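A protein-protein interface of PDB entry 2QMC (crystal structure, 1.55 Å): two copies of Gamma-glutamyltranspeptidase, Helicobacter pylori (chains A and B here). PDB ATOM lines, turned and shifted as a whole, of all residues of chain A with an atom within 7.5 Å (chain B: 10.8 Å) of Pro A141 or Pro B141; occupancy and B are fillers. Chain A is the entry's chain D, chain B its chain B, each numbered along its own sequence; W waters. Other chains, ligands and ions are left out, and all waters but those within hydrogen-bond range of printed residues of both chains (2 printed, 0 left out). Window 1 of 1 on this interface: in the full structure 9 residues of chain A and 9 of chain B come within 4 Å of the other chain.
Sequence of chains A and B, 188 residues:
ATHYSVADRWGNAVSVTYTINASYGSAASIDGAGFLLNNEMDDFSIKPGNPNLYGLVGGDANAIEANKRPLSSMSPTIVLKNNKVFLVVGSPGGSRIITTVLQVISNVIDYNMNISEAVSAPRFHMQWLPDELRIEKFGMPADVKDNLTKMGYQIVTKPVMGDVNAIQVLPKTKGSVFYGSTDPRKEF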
ATOM      1  N   ILE A 135       4.780  22.597  23.229  1.00  0.00           N
ATOM      2  CA  ILE A 135       3.645  23.447  23.619  1.00  0.00           C
ATOM      3  C   ILE A 135       3.511  23.523  25.146  1.00  0.00           C
ATOM      4  O   ILE A 135       4.202  22.780  25.895  1.00  0.00           O
ATOM      5  CB  ILE A 135       2.317  22.976  22.969  1.00  0.00           C
ATOM      6  CG1 ILE A 135       1.894  21.577  23.474  1.00  0.00           C
ATOM      7  CG2 ILE A 135       2.441  23.051  21.435  1.00  0.00           C
ATOM      8  CD1 ILE A 135       0.431  21.232  23.221  1.00  0.00           C
ATOM      9  N   PHE A 138      -2.686  23.515  28.535  1.00  0.00           N
ATOM     10  CA  PHE A 138      -3.837  24.353  28.179  1.00  0.00           C
ATOM     11  C   PHE A 138      -3.569  25.301  27.009  1.00  0.00           C
ATOM     12  O   PHE A 138      -4.385  26.171  26.725  1.00  0.00           O
ATOM     13  CB  PHE A 138      -4.321  25.151  29.399  1.00  0.00           C
ATOM     14  CG  PHE A 138      -4.395  24.339  30.665  1.00  0.00           C
ATOM     15  CD1 PHE A 138      -5.122  23.143  30.710  1.00  0.00           C
ATOM     16  CD2 PHE A 138      -3.732  24.768  31.814  1.00  0.00           C
ATOM     17  CE1 PHE A 138      -5.185  22.400  31.867  1.00  0.00           C
ATOM     18  CE2 PHE A 138      -3.777  24.015  32.987  1.00  0.00           C
ATOM     19  CZ  PHE A 138      -4.512  22.834  33.016  1.00  0.00           C
ATOM     20  N   GLY A 139      -2.450  25.154  26.328  1.00  0.00           N
ATOM     21  CA  GLY A 139      -2.068  26.147  25.337  1.00  0.00           C
ATOM     22  C   GLY A 139      -2.621  25.950  23.933  1.00  0.00           C
ATOM     23  O   GLY A 139      -2.660  26.899  23.132  1.00  0.00           O
ATOM     24  N   MET A 140      -2.993  24.717  23.628  1.00  0.00           N
ATOM     25  CA  MET A 140      -3.399  24.331  22.291  1.00  0.00           C
ATOM     26  C   MET A 140      -4.572  23.357  22.406  1.00  0.00           C
ATOM     27  O   MET A 140      -4.410  22.278  22.976  1.00  0.00           O
ATOM     28  CB  MET A 140      -2.243  23.603  21.618  1.00  0.00           C
ATOM     29  CG  MET A 140      -2.515  23.270  20.164  1.00  0.00           C
ATOM     30  SD  MET A 140      -1.047  22.633  19.350  1.00  0.00           S
ATOM     31  CE  MET A 140      -0.190  24.168  19.203  1.00  0.00           C
ATOM     32  N   PRO A 141      -5.740  23.714  21.842  1.00  0.00           N
ATOM     33  CA  PRO A 141      -6.872  22.805  21.945  1.00  0.00           C
ATOM     34  C   PRO A 141      -6.764  21.611  20.977  1.00  0.00           C
ATOM     35  O   PRO A 141      -6.018  21.668  19.995  1.00  0.00           O
ATOM     36  CB  PRO A 141      -8.075  23.698  21.577  1.00  0.00           C
ATOM     37  CG  PRO A 141      -7.510  24.673  20.635  1.00  0.00           C
ATOM     38  CD  PRO A 141      -6.091  24.948  21.103  1.00  0.00           C
ATOM     39  N   ALA A 142      -7.538  20.569  21.266  1.00  0.00           N
ATOM     40  CA  ALA A 142      -7.547  19.315  20.500  1.00  0.00           C
ATOM     41  C   ALA A 142      -7.629  19.518  19.007  1.00  0.00           C
ATOM     42  O   ALA A 142      -6.862  18.884  18.265  1.00  0.00           O
ATOM     43  CB  ALA A 142      -8.675  18.412  20.955  1.00  0.00           C
ATOM     44  N   ASP A 143      -8.513  20.416  18.553  1.00  0.00           N
ATOM     45  CA  ASP A 143      -8.718  20.621  17.112  1.00  0.00           C
ATOM     46  C   ASP A 143      -7.443  21.085  16.417  1.00  0.00           C
ATOM     47  O   ASP A 143      -7.126  20.643  15.300  1.00  0.00           O
ATOM     48  CB  ASP A 143      -9.820  21.669  16.870  1.00  0.00           C
ATOM     49  CG  ASP A 143     -11.147  21.298  17.520  1.00  0.00           C
ATOM     50  OD1 ASP A 143     -11.189  21.061  18.768  1.00  0.00           O
ATOM     51  OD2 ASP A 143     -12.186  21.255  16.792  1.00  0.00           O
ATOM     52  N   VAL A 144      -6.721  21.985  17.079  1.00  0.00           N
ATOM     53  CA  VAL A 144      -5.459  22.520  16.582  1.00  0.00           C
ATOM     54  C   VAL A 144      -4.367  21.448  16.648  1.00  0.00           C
ATOM     55  O   VAL A 144      -3.623  21.247  15.686  1.00  0.00           O
ATOM     56  CB  VAL A 144      -5.071  23.806  17.347  1.00  0.00           C
ATOM     57  CG1 VAL A 144      -3.708  24.283  16.906  1.00  0.00           C
ATOM     58  CG2 VAL A 144      -6.103  24.922  17.098  1.00  0.00           C
ATOM     59  N   LYS A 145      -4.293  20.738  17.771  1.00  0.00           N
ATOM     60  CA  LYS A 145      -3.317  19.650  17.912  1.00  0.00           C
ATOM     61  C   LYS A 145      -3.526  18.582  16.838  1.00  0.00           C
ATOM     62  O   LYS A 145      -2.555  18.120  16.231  1.00  0.00           O
ATOM     63  CB  LYS A 145      -3.391  19.006  19.302  1.00  0.00           C
ATOM     64  CG  LYS A 145      -3.012  19.971  20.453  1.00  0.00           C
ATOM     65  CD  LYS A 145      -2.729  19.229  21.757  1.00  0.00           C
ATOM     66  CE  LYS A 145      -3.937  18.697  22.436  1.00  0.00           C
ATOM     67  NZ  LYS A 145      -3.592  18.444  23.880  1.00  0.00           N
ATOM     68  N   ASP A 146      -4.784  18.208  16.600  1.00  0.00           N
ATOM     69  CA  ASP A 146      -5.137  17.223  15.564  1.00  0.00           C
ATOM     70  C   ASP A 146      -4.662  17.648  14.186  1.00  0.00           C
ATOM     71  O   ASP A 146      -4.034  16.864  13.451  1.00  0.00           O
ATOM     72  CB  ASP A 146      -6.655  17.025  15.524  1.00  0.00           C
ATOM     73  CG  ASP A 146      -7.163  16.234  16.696  1.00  0.00           C
ATOM     74  OD1 ASP A 146      -6.318  15.680  17.443  1.00  0.00           O
ATOM     75  OD2 ASP A 146      -8.405  16.189  16.869  1.00  0.00           O
ATOM     76  N   ASN A 147      -4.937  18.897  13.831  1.00  0.00           N
ATOM     77  CA  ASN A 147      -4.565  19.372  12.504  1.00  0.00           C
ATOM     78  C   ASN A 147      -3.059  19.470  12.335  1.00  0.00           C
ATOM     79  O   ASN A 147      -2.513  19.145  11.271  1.00  0.00           O
ATOM     80  CB  ASN A 147      -5.253  20.704  12.205  1.00  0.00           C
ATOM     81  CG  ASN A 147      -6.732  20.525  11.885  1.00  0.00           C
ATOM     82  OD1 ASN A 147      -7.166  19.436  11.513  1.00  0.00           O
ATOM     83  ND2 ASN A 147      -7.514  21.582  12.052  1.00  0.00           N
ATOM     84  N   LEU A 148      -2.360  19.887  13.383  1.00  0.00           N
ATOM     85  CA  LEU A 148      -0.902  19.952  13.297  1.00  0.00           C
ATOM     86  C   LEU A 148      -0.276  18.554  13.269  1.00  0.00           C
ATOM     87  O   LEU A 148       0.721  18.322  12.570  1.00  0.00           O
ATOM     88  CB  LEU A 148      -0.333  20.786  14.448  1.00  0.00           C
ATOM     89  CG  LEU A 148      -0.610  22.293  14.341  1.00  0.00           C
ATOM     90  CD1 LEU A 148      -0.357  22.986  15.694  1.00  0.00           C
ATOM     91  CD2 LEU A 148       0.157  22.959  13.231  1.00  0.00           C
ATOM     92  N   ILE A 155       3.826  16.552  18.736  1.00  0.00           N
ATOM     93  CA  ILE A 155       3.544  17.573  19.730  1.00  0.00           C
ATOM     94  C   ILE A 155       3.878  17.034  21.122  1.00  0.00           C
ATOM     95  O   ILE A 155       3.549  15.900  21.452  1.00  0.00           O
ATOM     96  CB  ILE A 155       2.076  18.028  19.624  1.00  0.00           C
ATOM     97  CG1 ILE A 155       1.787  18.588  18.222  1.00  0.00           C
ATOM     98  CG2 ILE A 155       1.759  19.025  20.714  1.00  0.00           C
ATOM     99  CD1 ILE A 155       0.300  18.804  17.929  1.00  0.00           C
ATOM    100  N   TYR B 111     -10.381  19.804  33.835  1.00  0.00           N
ATOM    101  CA  TYR B 111      -9.093  20.016  33.174  1.00  0.00           C
ATOM    102  C   TYR B 111      -7.928  20.188  34.142  1.00  0.00           C
ATOM    103  O   TYR B 111      -6.780  20.308  33.724  1.00  0.00           O
ATOM    104  CB  TYR B 111      -9.205  21.186  32.193  1.00  0.00           C
ATOM    105  CG  TYR B 111     -10.388  21.025  31.280  1.00  0.00           C
ATOM    106  CD1 TYR B 111     -10.611  19.814  30.591  1.00  0.00           C
ATOM    107  CD2 TYR B 111     -11.257  22.091  31.045  1.00  0.00           C
ATOM    108  CE1 TYR B 111     -11.701  19.663  29.747  1.00  0.00           C
ATOM    109  CE2 TYR B 111     -12.382  21.945  30.221  1.00  0.00           C
ATOM    110  CZ  TYR B 111     -12.579  20.738  29.555  1.00  0.00           C
ATOM    111  OH  TYR B 111     -13.678  20.641  28.736  1.00  0.00           O
ATOM    112  N   MET B 113      -7.149  22.711  35.993  1.00  0.00           N
ATOM    113  CA  MET B 113      -6.621  24.066  36.096  1.00  0.00           C
ATOM    114  C   MET B 113      -6.610  24.491  37.557  1.00  0.00           C
ATOM    115  O   MET B 113      -7.527  24.128  38.310  1.00  0.00           O
ATOM    116  CB  MET B 113      -7.471  25.041  35.295  1.00  0.00           C
ATOM    117  CG  MET B 113      -7.454  24.771  33.797  1.00  0.00           C
ATOM    118  SD  MET B 113      -8.089  26.211  32.951  1.00  0.00           S
ATOM    119  CE  MET B 113      -8.237  25.561  31.283  1.00  0.00           C
ATOM    120  N   PRO B 122     -10.431  31.646  28.444  1.00  0.00           N
ATOM    121  CA  PRO B 122     -11.539  32.208  27.657  1.00  0.00           C
ATOM    122  C   PRO B 122     -12.867  31.463  27.892  1.00  0.00           C
ATOM    123  O   PRO B 122     -12.880  30.253  28.141  1.00  0.00           O
ATOM    124  CB  PRO B 122     -11.080  32.034  26.209  1.00  0.00           C
ATOM    125  CG  PRO B 122      -9.553  32.059  26.304  1.00  0.00           C
ATOM    126  CD  PRO B 122      -9.239  31.368  27.615  1.00  0.00           C
ATOM    127  N   ARG B 123     -13.973  32.193  27.785  1.00  0.00           N
ATOM    128  CA  ARG B 123     -15.302  31.674  28.083  1.00  0.00           C
ATOM    129  C   ARG B 123     -16.165  31.771  26.824  1.00  0.00           C
ATOM    130  O   ARG B 123     -16.013  32.720  26.019  1.00  0.00           O
ATOM    131  CB  ARG B 123     -15.959  32.528  29.184  1.00  0.00           C
ATOM    132  CG  ARG B 123     -15.365  32.332  30.565  1.00  0.00           C
ATOM    133  CD  ARG B 123     -15.718  33.502  31.525  1.00  0.00           C
ATOM    134  NE  ARG B 123     -14.841  33.393  32.686  1.00  0.00           N
ATOM    135  CZ  ARG B 123     -14.591  34.354  33.564  1.00  0.00           C
ATOM    136  NH1 ARG B 123     -15.142  35.548  33.444  1.00  0.00           N
ATOM    137  NH2 ARG B 123     -13.736  34.100  34.558  1.00  0.00           N
ATOM    138  N   PHE B 124     -17.079  30.810  26.677  1.00  0.00           N
ATOM    139  CA  PHE B 124     -18.098  30.868  25.628  1.00  0.00           C
ATOM    140  C   PHE B 124     -19.482  30.897  26.263  1.00  0.00           C
ATOM    141  O   PHE B 124     -19.636  30.736  27.468  1.00  0.00           O
ATOM    142  CB  PHE B 124     -17.978  29.683  24.646  1.00  0.00           C
ATOM    143  CG  PHE B 124     -18.100  28.329  25.294  1.00  0.00           C
ATOM    144  CD1 PHE B 124     -16.974  27.664  25.779  1.00  0.00           C
ATOM    145  CD2 PHE B 124     -19.335  27.711  25.398  1.00  0.00           C
ATOM    146  CE1 PHE B 124     -17.094  26.410  26.386  1.00  0.00           C
ATOM    147  CE2 PHE B 124     -19.476  26.453  26.001  1.00  0.00           C
ATOM    148  CZ  PHE B 124     -18.351  25.795  26.496  1.00  0.00           C
ATOM    149  N   LEU B 133     -23.433  31.249  19.353  1.00  0.00           N
ATOM    150  CA  LEU B 133     -22.369  30.891  20.275  1.00  0.00           C
ATOM    151  C   LEU B 133     -21.498  32.117  20.495  1.00  0.00           C
ATOM    152  O   LEU B 133     -20.750  32.534  19.608  1.00  0.00           O
ATOM    153  CB  LEU B 133     -21.551  29.711  19.737  1.00  0.00           C
ATOM    154  CG  LEU B 133     -20.537  29.107  20.707  1.00  0.00           C
ATOM    155  CD1 LEU B 133     -21.236  28.544  21.905  1.00  0.00           C
ATOM    156  CD2 LEU B 133     -19.759  27.981  20.035  1.00  0.00           C
ATOM    157  N   ILE B 135     -18.522  34.248  21.973  1.00  0.00           N
ATOM    158  CA  ILE B 135     -17.146  34.001  22.410  1.00  0.00           C
ATOM    159  C   ILE B 135     -16.433  35.318  22.704  1.00  0.00           C
ATOM    160  O   ILE B 135     -16.975  36.413  22.461  1.00  0.00           O
ATOM    161  CB  ILE B 135     -16.338  33.158  21.366  1.00  0.00           C
ATOM    162  CG1 ILE B 135     -16.173  33.953  20.070  1.00  0.00           C
ATOM    163  CG2 ILE B 135     -16.986  31.786  21.151  1.00  0.00           C
ATOM    164  CD1 ILE B 135     -15.139  33.360  19.127  1.00  0.00           C
ATOM    165  N   GLU B 136     -15.194  35.207  23.172  1.00  0.00           N
ATOM    166  CA  GLU B 136     -14.363  36.356  23.530  1.00  0.00           C
ATOM    167  C   GLU B 136     -13.208  36.523  22.537  1.00  0.00           C
ATOM    168  O   GLU B 136     -12.772  35.555  21.906  1.00  0.00           O
ATOM    169  CB  GLU B 136     -13.828  36.167  24.958  1.00  0.00           C
ATOM    170  CG  GLU B 136     -14.941  36.049  26.041  1.00  0.00           C
ATOM    171  CD  GLU B 136     -14.389  35.843  27.427  1.00  0.00           C
ATOM    172  OE1 GLU B 136     -13.413  35.055  27.576  1.00  0.00           O
ATOM    173  OE2 GLU B 136     -14.922  36.466  28.359  1.00  0.00           O
ATOM    174  N   LYS B 137     -12.719  37.753  22.390  1.00  0.00           N
ATOM    175  CA  LYS B 137     -11.599  38.060  21.506  1.00  0.00           C
ATOM    176  C   LYS B 137     -10.393  37.205  21.928  1.00  0.00           C
ATOM    177  O   LYS B 137     -10.069  37.120  23.101  1.00  0.00           O
ATOM    178  CB  LYS B 137     -11.296  39.557  21.608  1.00  0.00           C
ATOM    179  CG  LYS B 137     -10.437  40.184  20.526  1.00  0.00           C
ATOM    180  CD  LYS B 137     -10.136  41.651  20.945  1.00  0.00           C
ATOM    181  CE  LYS B 137      -9.360  42.440  19.935  1.00  0.00           C
ATOM    182  NZ  LYS B 137      -8.729  43.636  20.601  1.00  0.00           N
ATOM    183  N   PHE B 138      -9.757  36.569  20.948  1.00  0.00           N
ATOM    184  CA  PHE B 138      -8.623  35.645  21.155  1.00  0.00           C
ATOM    185  C   PHE B 138      -8.962  34.358  21.900  1.00  0.00           C
ATOM    186  O   PHE B 138      -8.062  33.616  22.311  1.00  0.00           O
ATOM    187  CB  PHE B 138      -7.418  36.351  21.828  1.00  0.00           C
ATOM    188  CG  PHE B 138      -7.113  37.710  21.277  1.00  0.00           C
ATOM    189  CD1 PHE B 138      -6.776  37.865  19.936  1.00  0.00           C
ATOM    190  CD2 PHE B 138      -7.099  38.841  22.109  1.00  0.00           C
ATOM    191  CE1 PHE B 138      -6.468  39.128  19.396  1.00  0.00           C
ATOM    192  CE2 PHE B 138      -6.792  40.107  21.579  1.00  0.00           C
ATOM    193  CZ  PHE B 138      -6.478  40.243  20.235  1.00  0.00           C
ATOM    194  N   GLY B 139     -10.245  34.071  22.070  1.00  0.00           N
ATOM    195  CA  GLY B 139     -10.629  32.959  22.919  1.00  0.00           C
ATOM    196  C   GLY B 139     -10.786  31.639  22.201  1.00  0.00           C
ATOM    197  O   GLY B 139     -10.762  30.582  22.819  1.00  0.00           O
ATOM    198  N   MET B 140     -10.939  31.680  20.891  1.00  0.00           N
ATOM    199  CA  MET B 140     -11.167  30.460  20.137  1.00  0.00           C
ATOM    200  C   MET B 140     -10.384  30.533  18.830  1.00  0.00           C
ATOM    201  O   MET B 140     -10.626  31.454  18.046  1.00  0.00           O
ATOM    202  CB  MET B 140     -12.672  30.364  19.827  1.00  0.00           C
ATOM    203  CG  MET B 140     -13.042  29.117  19.098  1.00  0.00           C
ATOM    204  SD  MET B 140     -14.816  28.999  18.904  1.00  0.00           S
ATOM    205  CE  MET B 140     -15.155  28.639  20.587  1.00  0.00           C
ATOM    206  N   PRO B 141      -9.445  29.578  18.573  1.00  0.00           N
ATOM    207  CA  PRO B 141      -8.693  29.586  17.325  1.00  0.00           C
ATOM    208  C   PRO B 141      -9.502  29.144  16.115  1.00  0.00           C
ATOM    209  O   PRO B 141     -10.554  28.483  16.265  1.00  0.00           O
ATOM    210  CB  PRO B 141      -7.559  28.584  17.588  1.00  0.00           C
ATOM    211  CG  PRO B 141      -8.181  27.621  18.515  1.00  0.00           C
ATOM    212  CD  PRO B 141      -9.062  28.432  19.424  1.00  0.00           C
ATOM    213  N   ALA B 142      -9.009  29.528  14.945  1.00  0.00           N
ATOM    214  CA  ALA B 142      -9.643  29.231  13.660  1.00  0.00           C
ATOM    215  C   ALA B 142     -10.100  27.778  13.572  1.00  0.00           C
ATOM    216  O   ALA B 142     -11.241  27.517  13.195  1.00  0.00           O
ATOM    217  CB  ALA B 142      -8.692  29.571  12.502  1.00  0.00           C
ATOM    218  N   ASP B 143      -9.225  26.825  13.926  1.00  0.00           N
ATOM    219  CA  ASP B 143      -9.557  25.394  13.751  1.00  0.00           C
ATOM    220  C   ASP B 143     -10.794  25.004  14.538  1.00  0.00           C
ATOM    221  O   ASP B 143     -11.647  24.248  14.053  1.00  0.00           O
ATOM    222  CB  ASP B 143      -8.403  24.503  14.197  1.00  0.00           C
ATOM    223  CG  ASP B 143      -7.098  24.829  13.480  1.00  0.00           C
ATOM    224  OD1 ASP B 143      -6.674  26.016  13.483  1.00  0.00           O
ATOM    225  OD2 ASP B 143      -6.495  23.908  12.906  1.00  0.00           O
ATOM    226  N   VAL B 144     -10.918  25.545  15.748  1.00  0.00           N
ATOM    227  CA  VAL B 144     -12.036  25.239  16.623  1.00  0.00           C
ATOM    228  C   VAL B 144     -13.293  25.912  16.092  1.00  0.00           C
ATOM    229  O   VAL B 144     -14.347  25.278  16.012  1.00  0.00           O
ATOM    230  CB  VAL B 144     -11.721  25.650  18.079  1.00  0.00           C
ATOM    231  CG1 VAL B 144     -12.973  25.536  18.923  1.00  0.00           C
ATOM    232  CG2 VAL B 144     -10.652  24.745  18.684  1.00  0.00           C
ATOM    233  N   LYS B 145     -13.162  27.184  15.714  1.00  0.00           N
ATOM    234  CA  LYS B 145     -14.271  27.946  15.135  1.00  0.00           C
ATOM    235  C   LYS B 145     -14.798  27.254  13.882  1.00  0.00           C
ATOM    236  O   LYS B 145     -16.006  27.168  13.682  1.00  0.00           O
ATOM    237  CB  LYS B 145     -13.844  29.375  14.769  1.00  0.00           C
ATOM    238  CG  LYS B 145     -13.650  30.303  15.959  1.00  0.00           C
ATOM    239  CD  LYS B 145     -13.755  31.771  15.566  1.00  0.00           C
ATOM    240  CE  LYS B 145     -12.411  32.393  15.340  1.00  0.00           C
ATOM    241  NZ  LYS B 145     -12.499  33.898  15.322  1.00  0.00           N
ATOM    242  N   ASP B 146     -13.895  26.775  13.035  1.00  0.00           N
ATOM    243  CA  ASP B 146     -14.301  26.107  11.795  1.00  0.00           C
ATOM    244  C   ASP B 146     -15.156  24.873  12.085  1.00  0.00           C
ATOM    245  O   ASP B 146     -16.225  24.687  11.491  1.00  0.00           O
ATOM    246  CB  ASP B 146     -13.069  25.739  10.974  1.00  0.00           C
ATOM    247  CG  ASP B 146     -12.473  26.937  10.251  1.00  0.00           C
ATOM    248  OD1 ASP B 146     -13.095  28.024  10.290  1.00  0.00           O
ATOM    249  OD2 ASP B 146     -11.376  26.795   9.641  1.00  0.00           O
ATOM    250  N   ASN B 147     -14.677  24.039  13.005  1.00  0.00           N
ATOM    251  CA  ASN B 147     -15.401  22.830  13.377  1.00  0.00           C
ATOM    252  C   ASN B 147     -16.767  23.079  13.990  1.00  0.00           C
ATOM    253  O   ASN B 147     -17.746  22.408  13.648  1.00  0.00           O
ATOM    254  CB  ASN B 147     -14.530  21.926  14.235  1.00  0.00           C
ATOM    255  CG  ASN B 147     -13.468  21.229  13.408  1.00  0.00           C
ATOM    256  OD1 ASN B 147     -13.675  20.966  12.214  1.00  0.00           O
ATOM    257  ND2 ASN B 147     -12.347  20.895  14.034  1.00  0.00           N
ATOM    258  N   LEU B 148     -16.853  24.076  14.871  1.00  0.00           N
ATOM    259  CA  LEU B 148     -18.125  24.461  15.463  1.00  0.00           C
ATOM    260  C   LEU B 148     -19.074  25.067  14.428  1.00  0.00           C
ATOM    261  O   LEU B 148     -20.276  24.796  14.472  1.00  0.00           O
ATOM    262  CB  LEU B 148     -17.885  25.447  16.599  1.00  0.00           C
ATOM    263  CG  LEU B 148     -17.215  24.801  17.819  1.00  0.00           C
ATOM    264  CD1 LEU B 148     -16.775  25.881  18.789  1.00  0.00           C
ATOM    265  CD2 LEU B 148     -18.182  23.813  18.504  1.00  0.00           C
ATOM    266  N   THR B 149     -18.553  25.887  13.520  1.00  0.00           N
ATOM    267  CA  THR B 149     -19.366  26.471  12.445  1.00  0.00           C
ATOM    268  C   THR B 149     -19.943  25.373  11.558  1.00  0.00           C
ATOM    269  O   THR B 149     -21.127  25.439  11.170  1.00  0.00           O
ATOM    270  CB  THR B 149     -18.562  27.502  11.604  1.00  0.00           C
ATOM    271  OG1 THR B 149     -18.220  28.597  12.449  1.00  0.00           O
ATOM    272  CG2 THR B 149     -19.398  28.050  10.418  1.00  0.00           C
ATOM    273  N   LYS B 150     -19.136  24.347  11.285  1.00  0.00           N
ATOM    274  CA  LYS B 150     -19.599  23.208  10.486  1.00  0.00           C
ATOM    275  C   LYS B 150     -20.742  22.447  11.175  1.00  0.00           C
ATOM    276  O   LYS B 150     -21.662  21.948  10.513  1.00  0.00           O
ATOM    277  CB  LYS B 150     -18.425  22.291  10.144  1.00  0.00           C
ATOM    278  CG  LYS B 150     -17.553  22.844   9.038  1.00  0.00           C
ATOM    279  CD  LYS B 150     -16.291  22.023   8.863  1.00  0.00           C
ATOM    280  CE  LYS B 150     -15.435  22.647   7.764  1.00  0.00           C
ATOM    281  NZ  LYS B 150     -13.965  22.567   8.036  1.00  0.00           N
ATOM    282  N   ILE B 155     -21.151  31.724  15.291  1.00  0.00           N
ATOM    283  CA  ILE B 155     -20.208  32.215  16.281  1.00  0.00           C
ATOM    284  C   ILE B 155     -20.143  33.727  16.200  1.00  0.00           C
ATOM    285  O   ILE B 155     -20.007  34.278  15.113  1.00  0.00           O
ATOM    286  CB  ILE B 155     -18.826  31.587  16.053  1.00  0.00           C
ATOM    287  CG1 ILE B 155     -18.890  30.064  16.303  1.00  0.00           C
ATOM    288  CG2 ILE B 155     -17.762  32.291  16.902  1.00  0.00           C
ATOM    289  CD1 ILE B 155     -17.655  29.327  15.840  1.00  0.00           C
ATOM    290  N   THR B 157     -18.230  37.143  18.178  1.00  0.00           N
ATOM    291  CA  THR B 157     -17.293  37.679  19.186  1.00  0.00           C
ATOM    292  C   THR B 157     -17.900  38.937  19.804  1.00  0.00           C
ATOM    293  O   THR B 157     -18.267  39.887  19.089  1.00  0.00           O
ATOM    294  CB  THR B 157     -15.889  37.968  18.576  1.00  0.00           C
ATOM    295  OG1 THR B 157     -15.341  36.770  18.014  1.00  0.00           O
ATOM    296  CG2 THR B 157     -14.930  38.477  19.631  1.00  0.00           C
HETATM  297  O   HOH W   1      -9.536  19.435  13.770  1.00  0.00           O
HETATM  298  O   HOH W   2     -10.519  22.631  11.886  1.00  0.00           O
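Water W2 lies within hydrogen-bond range of the backbone carbonyl oxygen of Asp B143, the side-chain amide nitrogen of Asn A147 and the side-chain amide nitrogen of Asn B147.
Water W1 lies within hydrogen-bond range of O of Asp A143 (3.1 Å), ND2 of Asn B147 (3.2 Å) and OD1 of Asn A147 (3.3 Å).
Pro A141 touches its own counterpart, Pro B141.
Pro A141 touches Val B144, and with the chains exchanged Val A144 touches Pro B141.
Asp A143 touches Val B144, and with the chains exchanged Val A144 touches Asp B143.
Asp A143 touches Asn B147, and with the chains exchanged Asn A147 touches Asp B143.
Positions printed for both chains: 135, 138, 139, 140, 141, 142, 143, 144, 145, 146, 147, 148 and 155.
The side-chain amide nitrogen (ND2) of Asn A147 sits at hydrogen-bond distance from the backbone carbonyl oxygen (O) of Asp A143.
The backbone carbonyl oxygen of Asp B143 lies within hydrogen-bond range of the side-chain amide nitrogen of Asn B147, 3.4 Å away.
Of the 24 printed residues of chain B, 6 touch a printed residue of chain A.
Hydrophobic or aromatic side chains of chain B that line the printed part of chain A: Met B113, Pro B141 and Val B144.
Along chain B the printed residues that touch a printed residue of chain A span positions 111 to 147.
Printed residues of chain A that touch a printed residue of chain B: Phe A138, Pro A141, Asp A143, Val A144 and Asn A147.
Hydrophobic or aromatic side chains of chain A within 4 Å of the printed part of chain B: Phe A138, Pro A141 and Val A144.
Along chain A the printed residues that touch a printed residue of chain B span positions 138 to 147.
Among the printed residues, 9 pairs touch across the chains.
OD2 of Asp B143 sits at hydrogen-bond distance from ND2 of Asn A147, at 2.7 Å.
OD2 of Asp A143 is in hydrogen-bond range of ND2 of Asn B147 (2.8 Å).
Among the printed residues, merely in contact across the chains: Phe A138 with Tyr B111, Phe A138 with Met B113, Asp A143 with Val B144, Val A144 with Pro B141, Pro A141 with Pro B141, Pro A141 with Val B144 and Val A144 with Asp B143.
No residue of chain B comes within 4 Å of Gly A139.
Of chain B, only Pro B141 (3.7 Å) and Val B144 (3.7 Å) come within 4 Å of Pro A141.
No residue of chain B comes within 4 Å of Ala A142.
Of chain B, only Pro B141 and Asp B143 come within 4 Å of Val A144.
No residue of chain B comes within 4 Å of Lys A145.
Of the printed residues of chain B, Asn A147 touches Asp B143.
Printed residues of chain A within 4 Å of Met B113: Phe A138 (3.6 Å).
Leu B133 touches none of the printed residues of chain A.
Pro B141 touches just these residues of chain A: Pro A141 and Val A144.
Of the printed residues of chain A, Asp B143 touches Val A144 and Asn A147.
Of the printed residues of chain A, Asn B147 touches Asp A143 (2.8 Å).
Leu B148 touches none of the printed residues of chain A.
The nearest residue of chain A that does not touch Pro B141 is Asp A143 (6.4 Å).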
